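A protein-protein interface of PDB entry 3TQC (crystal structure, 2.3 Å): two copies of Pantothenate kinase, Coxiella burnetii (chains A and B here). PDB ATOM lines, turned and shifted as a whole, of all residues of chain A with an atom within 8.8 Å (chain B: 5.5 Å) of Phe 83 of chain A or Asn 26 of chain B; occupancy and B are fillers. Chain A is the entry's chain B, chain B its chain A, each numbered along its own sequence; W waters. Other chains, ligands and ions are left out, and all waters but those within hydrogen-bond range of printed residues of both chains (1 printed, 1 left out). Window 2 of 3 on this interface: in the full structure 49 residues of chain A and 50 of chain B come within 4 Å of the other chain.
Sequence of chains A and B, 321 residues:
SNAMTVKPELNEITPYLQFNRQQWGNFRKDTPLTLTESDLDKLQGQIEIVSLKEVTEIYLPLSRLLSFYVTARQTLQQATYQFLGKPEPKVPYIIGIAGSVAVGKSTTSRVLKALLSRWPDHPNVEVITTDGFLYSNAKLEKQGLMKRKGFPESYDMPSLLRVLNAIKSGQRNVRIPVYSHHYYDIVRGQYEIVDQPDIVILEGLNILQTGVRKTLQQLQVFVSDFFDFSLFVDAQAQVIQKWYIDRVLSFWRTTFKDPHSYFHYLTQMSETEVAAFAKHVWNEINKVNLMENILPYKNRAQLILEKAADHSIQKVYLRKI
NE2 of Gln 22 of chain B sits close to ND2 of Asn 26 of chain B, at 3.1 Å.
The backbone carbonyl oxygen (O) of Leu 76 of chain A sits at hydrogen-bond distance from the side-chain hydroxyl (OG1) of Thr 80 of chain A, at 2.7 Å.
OG1 of Thr 80 of chain A sits at hydrogen-bond distance from O of Gln 77 of chain A.
Among the printed residues, pairs that only touch across the chains: Phe 83 of chain A with Phe 68 of chain B (3.5 Å), Leu 76 of chain A with Phe 68 of chain B (3.5 Å), Thr 80 of chain A with Phe 68 of chain B (3.6 Å), Phe 83 of chain A with Pro 61 of chain B (3.7 Å), Phe 83 of chain A with Asn 26 of chain B (3.8 Å), Phe 83 of chain A with Arg 64 of chain B (3.8 Å), Leu 84 of chain A with Leu 65 of chain B (3.9 Å), Thr 80 of chain A with Leu 65 of chain B (3.9 Å) and Ala 79 of chain A with Phe 68 of chain B (3.95 Å).
Of the printed residues of chain B, Leu 76 of chain A touches Phe 68.
Printed residues of chain B within 4 Å of Ala 79 of chain A: Phe 68.
Printed residues of chain B within 4 Å of Phe 83 of chain A: Asn 26, Pro 61, Arg 64 and Phe 68.
Of the printed residues of chain B, Leu 84 of chain A touches Leu 65 (3.9 Å).
Of chain A, only Phe 83 comes within 4 Å of Asn 26 of chain B.
Of the printed residues of chain A, Pro 61 of chain B touches Phe 83.
Printed residues of chain A within 4 Å of Leu 65 of chain B: Thr 80 (3.9 Å) and Leu 84 (3.9 Å).
The nearest residue of chain B that does not touch Phe 83 of chain A is Leu 65 of chain B (4.05 Å).
The nearest residue of chain A that does not touch Asn 26 of chain B is Leu 84 of chain A (4.6 Å).
The nearest printed residue of chain B that does not touch Ala 79 of chain A is Leu 65 of chain B (7.0 Å).
Hydrophobic or aromatic side chains of chain A within 4 Å of the printed part of chain B: Leu 76, Ala 79, Phe 83 and Leu 84.
Of the 10 printed residues of chain B, 5 touch a printed residue of chain A.
Among the printed residues, 9 pairs touch across the chains.
Among the printed residues, no Asp or Glu carboxylate lies within 4 Å of a Lys or Arg side-chain nitrogen of the other chain.
No position is printed for both chains.
Of the 9 pairs that touch across the chains among the printed residues, none has its exchanged pair printed and touching as well.
Water W1 bridges the backbone carbonyl oxygen of Leu 84 of chain A and the backbone carbonyl oxygen of Gln 23 of chain B.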
ATOM      1  N   LEU A  76     -22.727  30.770  -5.811  1.00  0.00           N
ATOM      2  CA  LEU A  76     -23.325  29.439  -5.702  1.00  0.00           C
ATOM      3  C   LEU A  76     -24.073  29.058  -6.993  1.00  0.00           C
ATOM      4  O   LEU A  76     -23.926  27.949  -7.529  1.00  0.00           O
ATOM      5  CB  LEU A  76     -24.271  29.398  -4.501  1.00  0.00           C
ATOM      6  CG  LEU A  76     -25.006  28.078  -4.252  1.00  0.00           C
ATOM      7  CD1 LEU A  76     -23.965  27.008  -3.929  1.00  0.00           C
ATOM      8  CD2 LEU A  76     -26.083  28.210  -3.164  1.00  0.00           C
ATOM      9  N   GLN A  77     -24.887  29.984  -7.471  1.00  0.00           N
ATOM     10  CA  GLN A  77     -25.561  29.841  -8.753  1.00  0.00           C
ATOM     11  C   GLN A  77     -24.547  29.494  -9.852  1.00  0.00           C
ATOM     12  O   GLN A  77     -24.717  28.489 -10.541  1.00  0.00           O
ATOM     13  CB  GLN A  77     -26.336  31.128  -9.072  1.00  0.00           C
ATOM     14  CG  GLN A  77     -27.208  31.073 -10.321  1.00  0.00           C
ATOM     15  CD  GLN A  77     -26.432  31.317 -11.602  1.00  0.00           C
ATOM     16  OE1 GLN A  77     -25.458  32.059 -11.611  1.00  0.00           O
ATOM     17  NE2 GLN A  77     -26.844  30.665 -12.686  1.00  0.00           N
ATOM     18  N   GLN A  78     -23.484  30.290  -9.998  1.00  0.00           N
ATOM     19  CA  GLN A  78     -22.505  30.041 -11.049  1.00  0.00           C
ATOM     20  C   GLN A  78     -21.862  28.660 -10.923  1.00  0.00           C
ATOM     21  O   GLN A  78     -21.710  27.958 -11.927  1.00  0.00           O
ATOM     22  CB  GLN A  78     -21.396  31.111 -11.092  1.00  0.00           C
ATOM     23  CG  GLN A  78     -21.805  32.477 -11.677  1.00  0.00           C
ATOM     24  CD  GLN A  78     -20.756  33.084 -12.646  1.00  0.00           C
ATOM     25  OE1 GLN A  78     -19.684  32.494 -12.909  1.00  0.00           O
ATOM     26  NE2 GLN A  78     -21.076  34.271 -13.192  1.00  0.00           N
ATOM     27  N   ALA A  79     -21.475  28.277  -9.706  1.00  0.00           N
ATOM     28  CA  ALA A  79     -20.785  27.006  -9.509  1.00  0.00           C
ATOM     29  C   ALA A  79     -21.735  25.817  -9.698  1.00  0.00           C
ATOM     30  O   ALA A  79     -21.402  24.875 -10.413  1.00  0.00           O
ATOM     31  CB  ALA A  79     -20.109  26.963  -8.158  1.00  0.00           C
ATOM     32  N   THR A  80     -22.928  25.884  -9.121  1.00  0.00           N
ATOM     33  CA  THR A  80     -23.885  24.776  -9.217  1.00  0.00           C
ATOM     34  C   THR A  80     -24.439  24.602 -10.610  1.00  0.00           C
ATOM     35  O   THR A  80     -24.625  23.484 -11.052  1.00  0.00           O
ATOM     36  CB  THR A  80     -25.061  24.923  -8.239  1.00  0.00           C
ATOM     37  OG1 THR A  80     -25.707  26.185  -8.450  1.00  0.00           O
ATOM     38  CG2 THR A  80     -24.568  24.837  -6.834  1.00  0.00           C
ATOM     39  N   TYR A  81     -24.696  25.696 -11.319  1.00  0.00           N
ATOM     40  CA  TYR A  81     -25.185  25.577 -12.699  1.00  0.00           C
ATOM     41  C   TYR A  81     -24.107  25.028 -13.643  1.00  0.00           C
ATOM     42  O   TYR A  81     -24.412  24.275 -14.570  1.00  0.00           O
ATOM     43  CB  TYR A  81     -25.718  26.913 -13.209  1.00  0.00           C
ATOM     44  CG  TYR A  81     -27.075  27.270 -12.672  1.00  0.00           C
ATOM     45  CD1 TYR A  81     -28.050  27.788 -13.498  1.00  0.00           C
ATOM     46  CD2 TYR A  81     -27.397  27.067 -11.344  1.00  0.00           C
ATOM     47  CE1 TYR A  81     -29.302  28.117 -13.000  1.00  0.00           C
ATOM     48  CE2 TYR A  81     -28.621  27.399 -10.850  1.00  0.00           C
ATOM     49  CZ  TYR A  81     -29.574  27.921 -11.671  1.00  0.00           C
ATOM     50  OH  TYR A  81     -30.806  28.233 -11.148  1.00  0.00           O
ATOM     51  N   GLN A  82     -22.850  25.404 -13.414  1.00  0.00           N
ATOM     52  CA  GLN A  82     -21.738  24.803 -14.147  1.00  0.00           C
ATOM     53  C   GLN A  82     -21.775  23.282 -13.901  1.00  0.00           C
ATOM     54  O   GLN A  82     -21.770  22.487 -14.846  1.00  0.00           O
ATOM     55  CB  GLN A  82     -20.382  25.403 -13.700  1.00  0.00           C
ATOM     56  CG  GLN A  82     -19.155  24.881 -14.505  1.00  0.00           C
ATOM     57  CD  GLN A  82     -17.795  25.052 -13.793  1.00  0.00           C
ATOM     58  OE1 GLN A  82     -17.588  25.973 -13.002  1.00  0.00           O
ATOM     59  NE2 GLN A  82     -16.861  24.145 -14.091  1.00  0.00           N
ATOM     60  N   PHE A  83     -21.836  22.888 -12.626  1.00  0.00           N
ATOM     61  CA  PHE A  83     -21.848  21.475 -12.266  1.00  0.00           C
ATOM     62  C   PHE A  83     -23.099  20.752 -12.772  1.00  0.00           C
ATOM     63  O   PHE A  83     -23.019  19.618 -13.205  1.00  0.00           O
ATOM     64  CB  PHE A  83     -21.744  21.278 -10.753  1.00  0.00           C
ATOM     65  CG  PHE A  83     -21.999  19.864 -10.329  1.00  0.00           C
ATOM     66  CD1 PHE A  83     -21.126  18.857 -10.702  1.00  0.00           C
ATOM     67  CD2 PHE A  83     -23.127  19.531  -9.601  1.00  0.00           C
ATOM     68  CE1 PHE A  83     -21.358  17.534 -10.334  1.00  0.00           C
ATOM     69  CE2 PHE A  83     -23.374  18.208  -9.229  1.00  0.00           C
ATOM     70  CZ  PHE A  83     -22.493  17.211  -9.593  1.00  0.00           C
ATOM     71  N   LEU A  84     -24.255  21.402 -12.707  1.00  0.00           N
ATOM     72  CA  LEU A  84     -25.492  20.768 -13.166  1.00  0.00           C
ATOM     73  C   LEU A  84     -25.655  20.831 -14.676  1.00  0.00           C
ATOM     74  O   LEU A  84     -26.597  20.255 -15.211  1.00  0.00           O
ATOM     75  CB  LEU A  84     -26.709  21.406 -12.496  1.00  0.00           C
ATOM     76  CG  LEU A  84     -26.820  21.119 -11.008  1.00  0.00           C
ATOM     77  CD1 LEU A  84     -27.897  21.983 -10.393  1.00  0.00           C
ATOM     78  CD2 LEU A  84     -27.120  19.660 -10.807  1.00  0.00           C
ATOM     79  N   GLY A  85     -24.741  21.529 -15.351  1.00  0.00           N
ATOM     80  CA  GLY A  85     -24.816  21.710 -16.791  1.00  0.00           C
ATOM     81  C   GLY A  85     -26.073  22.447 -17.210  1.00  0.00           C
ATOM     82  O   GLY A  85     -26.752  22.038 -18.134  1.00  0.00           O
ATOM     83  N   LYS A  86     -26.387  23.532 -16.518  1.00  0.00           N
ATOM     84  CA  LYS A  86     -27.589  24.320 -16.815  1.00  0.00           C
ATOM     85  C   LYS A  86     -27.182  25.707 -17.296  1.00  0.00           C
ATOM     86  O   LYS A  86     -26.372  26.365 -16.660  1.00  0.00           O
ATOM     87  CB  LYS A  86     -28.498  24.414 -15.587  1.00  0.00           C
ATOM     88  CG  LYS A  86     -29.299  23.137 -15.288  1.00  0.00           C
ATOM     89  CD  LYS A  86     -30.384  22.880 -16.343  1.00  0.00           C
ATOM     90  CE  LYS A  86     -31.193  21.621 -16.082  1.00  0.00           C
ATOM     91  NZ  LYS A  86     -32.181  21.365 -17.180  1.00  0.00           N
ATOM     92  N   GLN B  22     -31.320  11.361 -17.548  1.00  0.00           N
ATOM     93  CA  GLN B  22     -30.175  11.607 -18.419  1.00  0.00           C
ATOM     94  C   GLN B  22     -29.548  12.978 -18.133  1.00  0.00           C
ATOM     95  O   GLN B  22     -28.315  13.119 -18.115  1.00  0.00           O
ATOM     96  CB  GLN B  22     -30.590  11.494 -19.894  1.00  0.00           C
ATOM     97  CG  GLN B  22     -29.484  11.836 -20.914  1.00  0.00           C
ATOM     98  CD  GLN B  22     -29.309  13.346 -21.140  1.00  0.00           C
ATOM     99  OE1 GLN B  22     -30.278  14.117 -21.064  1.00  0.00           O
ATOM    100  NE2 GLN B  22     -28.067  13.772 -21.411  1.00  0.00           N
ATOM    101  N   GLN B  23     -30.392  13.979 -17.906  1.00  0.00           N
ATOM    102  CA  GLN B  23     -29.909  15.335 -17.645  1.00  0.00           C
ATOM    103  C   GLN B  23     -29.211  15.417 -16.305  1.00  0.00           C
ATOM    104  O   GLN B  23     -28.265  16.182 -16.140  1.00  0.00           O
ATOM    105  CB  GLN B  23     -31.057  16.337 -17.673  1.00  0.00           C
ATOM    106  CG  GLN B  23     -31.529  16.682 -19.056  1.00  0.00           C
ATOM    107  CD  GLN B  23     -32.888  17.338 -19.060  1.00  0.00           C
ATOM    108  OE1 GLN B  23     -33.650  17.231 -18.102  1.00  0.00           O
ATOM    109  NE2 GLN B  23     -33.201  18.023 -20.145  1.00  0.00           N
ATOM    110  N   TRP B  24     -29.699  14.650 -15.334  1.00  0.00           N
ATOM    111  CA  TRP B  24     -29.021  14.537 -14.058  1.00  0.00           C
ATOM    112  C   TRP B  24     -27.617  13.921 -14.255  1.00  0.00           C
ATOM    113  O   TRP B  24     -26.665  14.330 -13.597  1.00  0.00           O
ATOM    114  CB  TRP B  24     -29.865  13.725 -13.068  1.00  0.00           C
ATOM    115  CG  TRP B  24     -29.373  13.818 -11.698  1.00  0.00           C
ATOM    116  CD1 TRP B  24     -28.666  12.873 -11.013  1.00  0.00           C
ATOM    117  CD2 TRP B  24     -29.512  14.934 -10.821  1.00  0.00           C
ATOM    118  NE1 TRP B  24     -28.371  13.332  -9.751  1.00  0.00           N
ATOM    119  CE2 TRP B  24     -28.870  14.599  -9.614  1.00  0.00           C
ATOM    120  CE3 TRP B  24     -30.125  16.185 -10.934  1.00  0.00           C
ATOM    121  CZ2 TRP B  24     -28.815  15.471  -8.540  1.00  0.00           C
ATOM    122  CZ3 TRP B  24     -30.069  17.046  -9.871  1.00  0.00           C
ATOM    123  CH2 TRP B  24     -29.422  16.685  -8.685  1.00  0.00           C
ATOM    124  N   GLY B  25     -27.488  12.980 -15.187  1.00  0.00           N
ATOM    125  CA  GLY B  25     -26.183  12.387 -15.528  1.00  0.00           C
ATOM    126  C   GLY B  25     -25.126  13.291 -16.171  1.00  0.00           C
ATOM    127  O   GLY B  25     -24.011  12.835 -16.435  1.00  0.00           O
ATOM    128  N   ASN B  26     -25.463  14.550 -16.465  1.00  0.00           N
ATOM    129  CA  ASN B  26     -24.449  15.577 -16.769  1.00  0.00           C
ATOM    130  C   ASN B  26     -24.134  16.389 -15.502  1.00  0.00           C
ATOM    131  O   ASN B  26     -23.112  16.182 -14.836  1.00  0.00           O
ATOM    132  CB  ASN B  26     -24.916  16.540 -17.874  1.00  0.00           C
ATOM    133  CG  ASN B  26     -25.179  15.845 -19.205  1.00  0.00           C
ATOM    134  OD1 ASN B  26     -24.355  15.891 -20.128  1.00  0.00           O
ATOM    135  ND2 ASN B  26     -26.339  15.208 -19.314  1.00  0.00           N
ATOM    136  N   LEU B  33     -16.074  12.143 -10.189  1.00  0.00           N
ATOM    137  CA  LEU B  33     -16.948  11.579  -9.158  1.00  0.00           C
ATOM    138  C   LEU B  33     -17.032  10.056  -9.234  1.00  0.00           C
ATOM    139  O   LEU B  33     -17.464   9.512 -10.244  1.00  0.00           O
ATOM    140  CB  LEU B  33     -18.355  12.168  -9.273  1.00  0.00           C
ATOM    141  CG  LEU B  33     -18.684  13.369  -8.387  1.00  0.00           C
ATOM    142  CD1 LEU B  33     -19.035  12.900  -7.000  1.00  0.00           C
ATOM    143  CD2 LEU B  33     -17.527  14.377  -8.357  1.00  0.00           C
ATOM    144  N   PRO B  61     -24.041  12.305  -7.133  1.00  0.00           N
ATOM    145  CA  PRO B  61     -24.107  13.678  -7.645  1.00  0.00           C
ATOM    146  C   PRO B  61     -24.961  14.621  -6.796  1.00  0.00           C
ATOM    147  O   PRO B  61     -24.621  15.792  -6.649  1.00  0.00           O
ATOM    148  CB  PRO B  61     -24.748  13.516  -9.024  1.00  0.00           C
ATOM    149  CG  PRO B  61     -24.509  12.105  -9.413  1.00  0.00           C
ATOM    150  CD  PRO B  61     -24.361  11.303  -8.159  1.00  0.00           C
ATOM    151  N   ARG B  64     -22.941  15.786  -4.096  1.00  0.00           N
ATOM    152  CA  ARG B  64     -22.000  16.810  -4.536  1.00  0.00           C
ATOM    153  C   ARG B  64     -22.707  18.138  -4.628  1.00  0.00           C
ATOM    154  O   ARG B  64     -22.172  19.153  -4.178  1.00  0.00           O
ATOM    155  CB  ARG B  64     -21.337  16.467  -5.881  1.00  0.00           C
ATOM    156  CG  ARG B  64     -20.399  17.566  -6.420  1.00  0.00           C
ATOM    157  CD  ARG B  64     -19.120  17.635  -5.583  1.00  0.00           C
ATOM    158  NE  ARG B  64     -18.227  18.772  -5.861  1.00  0.00           N
ATOM    159  CZ  ARG B  64     -18.299  19.963  -5.267  1.00  0.00           C
ATOM    160  NH1 ARG B  64     -19.263  20.231  -4.383  1.00  0.00           N
ATOM    161  NH2 ARG B  64     -17.419  20.904  -5.578  1.00  0.00           N
ATOM    162  N   LEU B  65     -23.901  18.137  -5.215  1.00  0.00           N
ATOM    163  CA  LEU B  65     -24.693  19.357  -5.336  1.00  0.00           C
ATOM    164  C   LEU B  65     -24.951  19.951  -3.959  1.00  0.00           C
ATOM    165  O   LEU B  65     -24.779  21.133  -3.739  1.00  0.00           O
ATOM    166  CB  LEU B  65     -26.012  19.065  -6.038  1.00  0.00           C
ATOM    167  CG  LEU B  65     -26.998  20.230  -6.155  1.00  0.00           C
ATOM    168  CD1 LEU B  65     -26.379  21.391  -6.892  1.00  0.00           C
ATOM    169  CD2 LEU B  65     -28.238  19.726  -6.865  1.00  0.00           C
ATOM    170  N   PHE B  68     -21.954  21.752  -2.551  1.00  0.00           N
ATOM    171  CA  PHE B  68     -21.817  23.136  -3.013  1.00  0.00           C
ATOM    172  C   PHE B  68     -22.556  24.100  -2.059  1.00  0.00           C
ATOM    173  O   PHE B  68     -22.008  25.123  -1.668  1.00  0.00           O
ATOM    174  CB  PHE B  68     -22.357  23.315  -4.445  1.00  0.00           C
ATOM    175  CG  PHE B  68     -21.404  22.899  -5.554  1.00  0.00           C
ATOM    176  CD1 PHE B  68     -20.270  23.636  -5.832  1.00  0.00           C
ATOM    177  CD2 PHE B  68     -21.706  21.828  -6.368  1.00  0.00           C
ATOM    178  CE1 PHE B  68     -19.403  23.282  -6.897  1.00  0.00           C
ATOM    179  CE2 PHE B  68     -20.866  21.447  -7.405  1.00  0.00           C
ATOM    180  CZ  PHE B  68     -19.706  22.187  -7.682  1.00  0.00           C
HETATM  181  O   HOH W   1     -28.165  18.933 -17.146  1.00  0.00           O
